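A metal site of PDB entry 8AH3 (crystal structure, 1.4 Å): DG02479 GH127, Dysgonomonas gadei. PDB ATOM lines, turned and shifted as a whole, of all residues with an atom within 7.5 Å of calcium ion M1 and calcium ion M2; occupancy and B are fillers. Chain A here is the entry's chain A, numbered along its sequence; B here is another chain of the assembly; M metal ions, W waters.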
ATOM      1  N   SER A  27      13.198  28.222  -7.331  1.00  0.00           N
ATOM      2  CA  SER A  27      13.504  29.422  -8.089  1.00  0.00           C
ATOM      3  C   SER A  27      14.017  29.102  -9.503  1.00  0.00           C
ATOM      4  O   SER A  27      14.549  29.966 -10.186  1.00  0.00           O
ATOM      5  CB  SER A  27      14.409  30.323  -7.254  1.00  0.00           C
ATOM      6  OG  SER A  27      15.627  29.676  -6.915  1.00  0.00           O
ATOM      7  N   ASN A  28      13.880  27.850 -10.001  1.00  0.00           N
ATOM      8  CA  ASN A  28      14.282  27.535 -11.363  1.00  0.00           C
ATOM      9  C   ASN A  28      13.751  28.576 -12.374  1.00  0.00           C
ATOM     10  O   ASN A  28      12.608  28.987 -12.279  1.00  0.00           O
ATOM     11  CB  ASN A  28      13.776  26.155 -11.755  1.00  0.00           C
ATOM     12  CG  ASN A  28      14.141  25.751 -13.148  1.00  0.00           C
ATOM     13  OD1 ASN A  28      15.247  25.248 -13.427  1.00  0.00           O
ATOM     14  ND2 ASN A  28      13.187  25.960 -14.031  1.00  0.00           N
ATOM     15  N   ASP A  29      14.607  28.953 -13.339  1.00  0.00           N
ATOM     16  CA  ASP A  29      14.265  29.922 -14.390  1.00  0.00           C
ATOM     17  C   ASP A  29      13.339  29.223 -15.383  1.00  0.00           C
ATOM     18  O   ASP A  29      13.770  28.329 -16.110  1.00  0.00           O
ATOM     19  CB  ASP A  29      15.542  30.377 -15.108  1.00  0.00           C
ATOM     20  CG  ASP A  29      15.343  31.414 -16.221  1.00  0.00           C
ATOM     21  OD1 ASP A  29      14.198  31.621 -16.659  1.00  0.00           O
ATOM     22  OD2 ASP A  29      16.362  32.029 -16.614  1.00  0.00           O
ATOM     23  N   PRO A  30      12.047  29.591 -15.466  1.00  0.00           N
ATOM     24  CA  PRO A  30      11.130  28.876 -16.361  1.00  0.00           C
ATOM     25  C   PRO A  30      11.477  29.024 -17.856  1.00  0.00           C
ATOM     26  O   PRO A  30      11.153  28.135 -18.632  1.00  0.00           O
ATOM     27  CB  PRO A  30       9.756  29.436 -15.987  1.00  0.00           C
ATOM     28  CG  PRO A  30      10.030  30.800 -15.392  1.00  0.00           C
ATOM     29  CD  PRO A  30      11.376  30.667 -14.696  1.00  0.00           C
ATOM     30  N   ALA A  31      12.236  30.074 -18.223  1.00  0.00           N
ATOM     31  CA  ALA A  31      12.657  30.256 -19.607  1.00  0.00           C
ATOM     32  C   ALA A  31      13.843  29.369 -19.967  1.00  0.00           C
ATOM     33  O   ALA A  31      14.313  29.410 -21.104  1.00  0.00           O
ATOM     34  CB  ALA A  31      12.960  31.714 -19.886  1.00  0.00           C
ATOM     35  N   GLY A  32      14.424  28.596 -18.998  1.00  0.00           N
ATOM     36  CA  GLY A  32      15.507  27.715 -19.347  1.00  0.00           C
ATOM     37  C   GLY A  32      16.917  28.277 -19.093  1.00  0.00           C
ATOM     38  O   GLY A  32      17.899  27.613 -19.417  1.00  0.00           O
ATOM     39  N   GLY A  33      16.984  29.490 -18.565  1.00  0.00           N
ATOM     40  CA  GLY A  33      18.255  30.195 -18.549  1.00  0.00           C
ATOM     41  C   GLY A  33      18.936  30.114 -17.171  1.00  0.00           C
ATOM     42  O   GLY A  33      18.725  29.160 -16.412  1.00  0.00           O
ATOM     43  N   VAL A  34      19.707  31.164 -16.869  1.00  0.00           N
ATOM     44  CA  VAL A  34      20.618  31.174 -15.732  1.00  0.00           C
ATOM     45  C   VAL A  34      19.984  31.881 -14.559  1.00  0.00           C
ATOM     46  O   VAL A  34      20.585  31.889 -13.464  1.00  0.00           O
ATOM     47  CB  VAL A  34      21.966  31.867 -16.082  1.00  0.00           C
ATOM     48  CG1 VAL A  34      22.693  31.152 -17.163  1.00  0.00           C
ATOM     49  CG2 VAL A  34      21.782  33.370 -16.377  1.00  0.00           C
ATOM     50  N   LEU A  35      18.784  32.473 -14.704  1.00  0.00           N
ATOM     51  CA  LEU A  35      18.187  33.262 -13.633  1.00  0.00           C
ATOM     52  C   LEU A  35      17.387  32.343 -12.690  1.00  0.00           C
ATOM     53  O   LEU A  35      16.166  32.478 -12.522  1.00  0.00           O
ATOM     54  CB  LEU A  35      17.287  34.378 -14.159  1.00  0.00           C
ATOM     55  CG  LEU A  35      17.981  35.454 -15.015  1.00  0.00           C
ATOM     56  CD1 LEU A  35      16.947  36.456 -15.516  1.00  0.00           C
ATOM     57  CD2 LEU A  35      19.072  36.147 -14.221  1.00  0.00           C
ATOM     58  N   ASP A  36      18.118  31.403 -12.089  1.00  0.00           N
ATOM     59  CA  ASP A  36      17.548  30.344 -11.252  1.00  0.00           C
ATOM     60  C   ASP A  36      17.368  30.779  -9.810  1.00  0.00           C
ATOM     61  O   ASP A  36      17.448  29.963  -8.893  1.00  0.00           O
ATOM     62  CB  ASP A  36      18.423  29.094 -11.377  1.00  0.00           C
ATOM     63  CG  ASP A  36      18.481  28.474 -12.746  1.00  0.00           C
ATOM     64  OD1 ASP A  36      17.364  28.312 -13.400  1.00  0.00           O
ATOM     65  OD2 ASP A  36      19.568  28.123 -13.202  1.00  0.00           O
ATOM     66  N   TYR A 152      17.776  32.058  -3.756  1.00  0.00           N
ATOM     67  CA  TYR A 152      17.672  30.731  -4.361  1.00  0.00           C
ATOM     68  C   TYR A 152      16.978  29.826  -3.355  1.00  0.00           C
ATOM     69  O   TYR A 152      17.245  29.912  -2.145  1.00  0.00           O
ATOM     70  CB  TYR A 152      19.065  30.138  -4.590  1.00  0.00           C
ATOM     71  CG  TYR A 152      19.884  30.680  -5.729  1.00  0.00           C
ATOM     72  CD1 TYR A 152      20.633  31.842  -5.578  1.00  0.00           C
ATOM     73  CD2 TYR A 152      19.964  29.999  -6.917  1.00  0.00           C
ATOM     74  CE1 TYR A 152      21.450  32.300  -6.588  1.00  0.00           C
ATOM     75  CE2 TYR A 152      20.774  30.447  -7.948  1.00  0.00           C
ATOM     76  CZ  TYR A 152      21.457  31.632  -7.787  1.00  0.00           C
ATOM     77  OH  TYR A 152      22.250  32.022  -8.796  1.00  0.00           O
ATOM     78  N   GLU B 188      30.031  28.642 -20.020  1.00  0.00           N
ATOM     79  CA  GLU B 188      29.717  28.820 -18.617  1.00  0.00           C
ATOM     80  C   GLU B 188      30.084  30.216 -18.128  1.00  0.00           C
ATOM     81  O   GLU B 188      31.152  30.752 -18.518  1.00  0.00           O
ATOM     82  CB  GLU B 188      30.474  27.808 -17.776  1.00  0.00           C
ATOM     83  CG  GLU B 188      29.951  27.750 -16.352  1.00  0.00           C
ATOM     84  CD  GLU B 188      28.438  27.487 -16.384  1.00  0.00           C
ATOM     85  OE1 GLU B 188      28.103  26.290 -16.569  1.00  0.00           O
ATOM     86  OE2 GLU B 188      27.667  28.448 -16.204  1.00  0.00           O
ATOM     87  N   ASN B 197      19.559  28.840 -23.627  1.00  0.00           N
ATOM     88  CA  ASN B 197      18.547  28.273 -22.749  1.00  0.00           C
ATOM     89  C   ASN B 197      18.470  26.743 -22.911  1.00  0.00           C
ATOM     90  O   ASN B 197      18.857  26.144 -23.911  1.00  0.00           O
ATOM     91  CB  ASN B 197      17.179  28.891 -23.017  1.00  0.00           C
ATOM     92  CG  ASN B 197      17.080  30.356 -22.666  1.00  0.00           C
ATOM     93  OD1 ASN B 197      17.578  30.814 -21.640  1.00  0.00           O
ATOM     94  ND2 ASN B 197      16.429  31.118 -23.527  1.00  0.00           N
ATOM     95  N   ASN B 198      17.894  26.078 -21.877  1.00  0.00           N
ATOM     96  CA  ASN B 198      17.629  24.647 -21.913  1.00  0.00           C
ATOM     97  C   ASN B 198      16.271  24.433 -21.240  1.00  0.00           C
ATOM     98  O   ASN B 198      16.178  24.324 -20.007  1.00  0.00           O
ATOM     99  CB  ASN B 198      18.705  23.870 -21.156  1.00  0.00           C
ATOM    100  CG  ASN B 198      18.370  22.406 -20.977  1.00  0.00           C
ATOM    101  OD1 ASN B 198      17.643  21.832 -21.796  1.00  0.00           O
ATOM    102  ND2 ASN B 198      18.949  21.779 -19.954  1.00  0.00           N
ATOM    103  N   GLY B 232      29.352  23.423 -11.702  1.00  0.00           N
ATOM    104  CA  GLY B 232      28.124  23.025 -11.041  1.00  0.00           C
ATOM    105  C   GLY B 232      26.917  23.937 -11.225  1.00  0.00           C
ATOM    106  O   GLY B 232      26.006  23.930 -10.376  1.00  0.00           O
ATOM    107  N   GLU B 233      26.859  24.701 -12.325  1.00  0.00           N
ATOM    108  CA  GLU B 233      25.706  25.566 -12.543  1.00  0.00           C
ATOM    109  C   GLU B 233      24.476  24.756 -13.037  1.00  0.00           C
ATOM    110  O   GLU B 233      23.380  25.298 -13.028  1.00  0.00           O
ATOM    111  CB  GLU B 233      25.961  26.676 -13.576  1.00  0.00           C
ATOM    112  CG  GLU B 233      26.968  27.723 -13.102  1.00  0.00           C
ATOM    113  CD  GLU B 233      26.562  28.672 -11.992  1.00  0.00           C
ATOM    114  OE1 GLU B 233      25.352  28.878 -11.763  1.00  0.00           O
ATOM    115  OE2 GLU B 233      27.488  29.219 -11.298  1.00  0.00           O
ATOM    116  N   GLY B 234      24.661  23.508 -13.372  1.00  0.00           N
ATOM    117  CA  GLY B 234      23.595  22.720 -13.980  1.00  0.00           C
ATOM    118  C   GLY B 234      22.470  22.329 -13.012  1.00  0.00           C
ATOM    119  O   GLY B 234      22.710  21.883 -11.896  1.00  0.00           O
ATOM    120  N   ASP B 235      21.229  22.410 -13.492  1.00  0.00           N
ATOM    121  CA  ASP B 235      20.022  22.136 -12.730  1.00  0.00           C
ATOM    122  C   ASP B 235      19.620  20.664 -12.822  1.00  0.00           C
ATOM    123  O   ASP B 235      19.752  20.043 -13.862  1.00  0.00           O
ATOM    124  CB  ASP B 235      18.852  22.908 -13.348  1.00  0.00           C
ATOM    125  CG  ASP B 235      19.067  24.415 -13.467  1.00  0.00           C
ATOM    126  OD1 ASP B 235      20.008  24.954 -12.806  1.00  0.00           O
ATOM    127  OD2 ASP B 235      18.253  25.083 -14.186  1.00  0.00           O
ATOM    128  N   ASP B 236      19.090  20.140 -11.717  1.00  0.00           N
ATOM    129  CA  ASP B 236      18.490  18.810 -11.696  1.00  0.00           C
ATOM    130  C   ASP B 236      17.054  18.904 -12.247  1.00  0.00           C
ATOM    131  O   ASP B 236      16.340  19.865 -11.991  1.00  0.00           O
ATOM    132  CB  ASP B 236      18.533  18.232 -10.278  1.00  0.00           C
ATOM    133  CG  ASP B 236      17.949  19.111  -9.234  1.00  0.00           C
ATOM    134  OD1 ASP B 236      18.478  20.222  -9.061  1.00  0.00           O
ATOM    135  OD2 ASP B 236      16.947  18.681  -8.558  1.00  0.00           O
ATOM    136  N   PHE B 237      16.669  17.866 -12.981  1.00  0.00           N
ATOM    137  CA  PHE B 237      15.341  17.659 -13.571  1.00  0.00           C
ATOM    138  C   PHE B 237      14.876  16.245 -13.169  1.00  0.00           C
ATOM    139  O   PHE B 237      15.594  15.277 -13.375  1.00  0.00           O
ATOM    140  CB  PHE B 237      15.428  17.628 -15.111  1.00  0.00           C
ATOM    141  CG  PHE B 237      15.612  18.922 -15.842  1.00  0.00           C
ATOM    142  CD1 PHE B 237      16.714  19.738 -15.609  1.00  0.00           C
ATOM    143  CD2 PHE B 237      14.816  19.236 -16.927  1.00  0.00           C
ATOM    144  CE1 PHE B 237      16.917  20.922 -16.310  1.00  0.00           C
ATOM    145  CE2 PHE B 237      15.043  20.393 -17.654  1.00  0.00           C
ATOM    146  CZ  PHE B 237      16.108  21.215 -17.376  1.00  0.00           C
ATOM    147  N   GLY B 250      15.469  21.959 -10.354  1.00  0.00           N
ATOM    148  CA  GLY B 250      16.432  22.579  -9.438  1.00  0.00           C
ATOM    149  C   GLY B 250      17.055  23.837 -10.033  1.00  0.00           C
ATOM    150  O   GLY B 250      16.631  24.347 -11.060  1.00  0.00           O
ATOM    151  N   THR B 251      18.145  24.292  -9.390  1.00  0.00           N
ATOM    152  CA  THR B 251      18.729  25.598  -9.710  1.00  0.00           C
ATOM    153  C   THR B 251      20.234  25.492  -9.971  1.00  0.00           C
ATOM    154  O   THR B 251      20.838  26.418 -10.528  1.00  0.00           O
ATOM    155  CB  THR B 251      18.451  26.582  -8.586  1.00  0.00           C
ATOM    156  OG1 THR B 251      18.989  26.094  -7.353  1.00  0.00           O
ATOM    157  CG2 THR B 251      16.978  26.828  -8.385  1.00  0.00           C
ATOM    158  N   GLY B 252      20.859  24.393  -9.549  1.00  0.00           N
ATOM    159  CA  GLY B 252      22.299  24.221  -9.642  1.00  0.00           C
ATOM    160  C   GLY B 252      22.687  22.907  -8.988  1.00  0.00           C
ATOM    161  O   GLY B 252      21.867  22.255  -8.346  1.00  0.00           O
ATOM    162  N   THR B 253      23.944  22.507  -9.204  1.00  0.00           N
ATOM    163  CA  THR B 253      24.418  21.215  -8.737  1.00  0.00           C
ATOM    164  C   THR B 253      24.796  21.241  -7.253  1.00  0.00           C
ATOM    165  O   THR B 253      24.385  20.360  -6.483  1.00  0.00           O
ATOM    166  CB  THR B 253      25.564  20.722  -9.619  1.00  0.00           C
ATOM    167  OG1 THR B 253      25.006  20.614 -10.948  1.00  0.00           O
ATOM    168  CG2 THR B 253      26.174  19.424  -9.136  1.00  0.00           C
ATOM    169  N   GLU B 254      25.521  22.275  -6.816  1.00  0.00           N
ATOM    170  CA  GLU B 254      25.779  22.391  -5.386  1.00  0.00           C
ATOM    171  C   GLU B 254      24.437  22.521  -4.658  1.00  0.00           C
ATOM    172  O   GLU B 254      24.253  22.012  -3.543  1.00  0.00           O
ATOM    173  CB  GLU B 254      26.789  23.519  -5.083  1.00  0.00           C
ATOM    174  CG  GLU B 254      26.259  24.950  -5.053  1.00  0.00           C
ATOM    175  CD  GLU B 254      26.140  25.667  -6.389  1.00  0.00           C
ATOM    176  OE1 GLU B 254      25.543  25.094  -7.353  1.00  0.00           O
ATOM    177  OE2 GLU B 254      26.678  26.798  -6.509  1.00  0.00           O
ATOM    178  N   ASP B 255      23.472  23.231  -5.274  1.00  0.00           N
ATOM    179  CA  ASP B 255      22.156  23.487  -4.711  1.00  0.00           C
ATOM    180  C   ASP B 255      21.399  22.170  -4.458  1.00  0.00           C
ATOM    181  O   ASP B 255      20.851  21.966  -3.361  1.00  0.00           O
ATOM    182  CB  ASP B 255      21.371  24.437  -5.641  1.00  0.00           C
ATOM    183  CG  ASP B 255      22.061  25.749  -6.021  1.00  0.00           C
ATOM    184  OD1 ASP B 255      23.110  26.103  -5.420  1.00  0.00           O
ATOM    185  OD2 ASP B 255      21.533  26.461  -6.902  1.00  0.00           O
ATOM    186  N   GLU B 309      21.856  19.029 -15.703  1.00  0.00           N
ATOM    187  CA  GLU B 309      22.643  19.691 -16.738  1.00  0.00           C
ATOM    188  C   GLU B 309      24.142  19.527 -16.408  1.00  0.00           C
ATOM    189  O   GLU B 309      24.509  19.565 -15.225  1.00  0.00           O
ATOM    190  CB  GLU B 309      22.307  21.152 -16.792  1.00  0.00           C
ATOM    191  CG  GLU B 309      20.870  21.517 -17.024  1.00  0.00           C
ATOM    192  CD  GLU B 309      20.683  23.016 -17.035  1.00  0.00           C
ATOM    193  OE1 GLU B 309      20.992  23.663 -16.052  1.00  0.00           O
ATOM    194  OE2 GLU B 309      20.216  23.568 -18.091  1.00  0.00           O
ATOM    195  N   GLY B 311      27.031  21.598 -16.626  1.00  0.00           N
ATOM    196  CA  GLY B 311      27.138  23.030 -16.788  1.00  0.00           C
ATOM    197  C   GLY B 311      25.805  23.640 -17.153  1.00  0.00           C
ATOM    198  O   GLY B 311      24.865  22.899 -17.541  1.00  0.00           O
ATOM    199  N   HIS B 312      25.685  24.953 -17.038  1.00  0.00           N
ATOM    200  CA  HIS B 312      24.462  25.633 -17.442  1.00  0.00           C
ATOM    201  C   HIS B 312      24.130  25.298 -18.900  1.00  0.00           C
ATOM    202  O   HIS B 312      24.992  25.337 -19.790  1.00  0.00           O
ATOM    203  CB  HIS B 312      24.512  27.151 -17.279  1.00  0.00           C
ATOM    204  CG  HIS B 312      23.317  27.761 -17.931  1.00  0.00           C
ATOM    205  ND1 HIS B 312      22.037  27.658 -17.399  1.00  0.00           N
ATOM    206  CD2 HIS B 312      23.209  28.296 -19.177  1.00  0.00           C
ATOM    207  CE1 HIS B 312      21.167  28.156 -18.294  1.00  0.00           C
ATOM    208  NE2 HIS B 312      21.883  28.543 -19.407  1.00  0.00           N
ATOM    209  N   ALA B 313      22.861  24.840 -19.120  1.00  0.00           N
ATOM    210  CA  ALA B 313      22.450  24.372 -20.440  1.00  0.00           C
ATOM    211  C   ALA B 313      23.431  23.417 -21.097  1.00  0.00           C
ATOM    212  O   ALA B 313      23.589  23.412 -22.334  1.00  0.00           O
ATOM    213  CB  ALA B 313      22.202  25.569 -21.350  1.00  0.00           C
HETATM  214 CA    CA M   1      21.470  26.754 -12.822  1.00  0.00          CA
HETATM  215 CA    CA M   2      18.445  27.078 -15.241  1.00  0.00          CA
HETATM  216  O   HOH W   1      18.759  25.910 -17.396  1.00  0.00           O
HETATM  217  O   HOH W   2      22.652  28.367 -14.298  1.00  0.00           O
HETATM  218  O   HOH W   3      22.867  28.159 -11.360  1.00  0.00           O
HETATM  219  O   HOH W   4      20.903  26.272 -15.290  1.00  0.00           O
HETATM  220  O   HOH W   5      16.223  26.883 -16.009  1.00  0.00           O
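The side-chain carboxylate (OD2) of Asp 235 of chain B is bound to calcium ion M2, at 2.3 Å.
Calcium ion M2 is bound by water W5 (2.4 Å).
The backbone carbonyl oxygen (O) of Gly 33 is bound to calcium ion M2.
OD1 of Asp 36 is bound to calcium ion M2 (2.5 Å).
Water W1 is bound to calcium ion M2 (2.5 Å).
OD2 of Asp 36 is bound to calcium ion M2 (2.6 Å).
Water W4 is bound to calcium ion M2.
Water W4 lies within hydrogen-bond range of OE1 of Glu 309 of chain B and ND1 of His 312 of chain B.
Water W1 lies within hydrogen-bond range of the backbone carbonyl oxygen (O) of Gly 32 (2.8 Å) and the side-chain carboxylate (OE2) of Glu 309 of chain B (2.8 Å).
Water W5 lies within hydrogen-bond range of O of Asp 29 (2.8 Å) and OD1 of Asn 28 (3.2 Å).
OG of Ser 27 sits at hydrogen-bond distance from O of Asp 36, at 2.7 Å.
OD1 of Asp 36 lies close to N of Asp 29, at 2.8 Å.
OD2 of Asp 29 lies close to N of Gly 33, at 3.3 Å.
N of Gly 252 of chain B sits close to OD1 of Asp 235 of chain B (3.4 Å).
The backbone NH (N) of Asp 235 of chain B lies within hydrogen-bond range of the side-chain carboxylate (OE1) of Glu 309 of chain B, at 2.9 Å.
The backbone NH of Gly 33 sits close to the side-chain amide oxygen of Asn 197 of chain B (3.4 Å).
The side-chain hydroxyl (OG1) of Thr 251 of chain B sits at hydrogen-bond distance from the side-chain carboxylate (OD2) of Asp 255 of chain B (2.6 Å).
The side-chain carboxylate of Asp 235 of chain B sits close to the side-chain amide oxygen of Asn 28 (3.1 Å).
Within 4 Å of calcium ion M1: Asp 36, Glu 233 of chain B, Asp 235 of chain B and Thr 251 of chain B.
The nearest printed residue that does not touch calcium ion M1 is Gly 252 of chain B (4.1 Å).
Calcium ion M1 is bound by the side-chain carboxylate (OD1) of Asp 235 of chain B (2.3 Å).
Calcium ion M1 is bound by the side-chain carboxylate (OD2) of Asp 36 (2.4 Å).
O of Thr 251 of chain B binds calcium ion M1, at 2.4 Å.
O of Glu 233 of chain B binds calcium ion M1 (2.4 Å).
Water W3 is bound to calcium ion M1 (2.5 Å).
Calcium ion M1 is bound by water W2.
Calcium ion M1 is bound by water W4 (2.6 Å).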
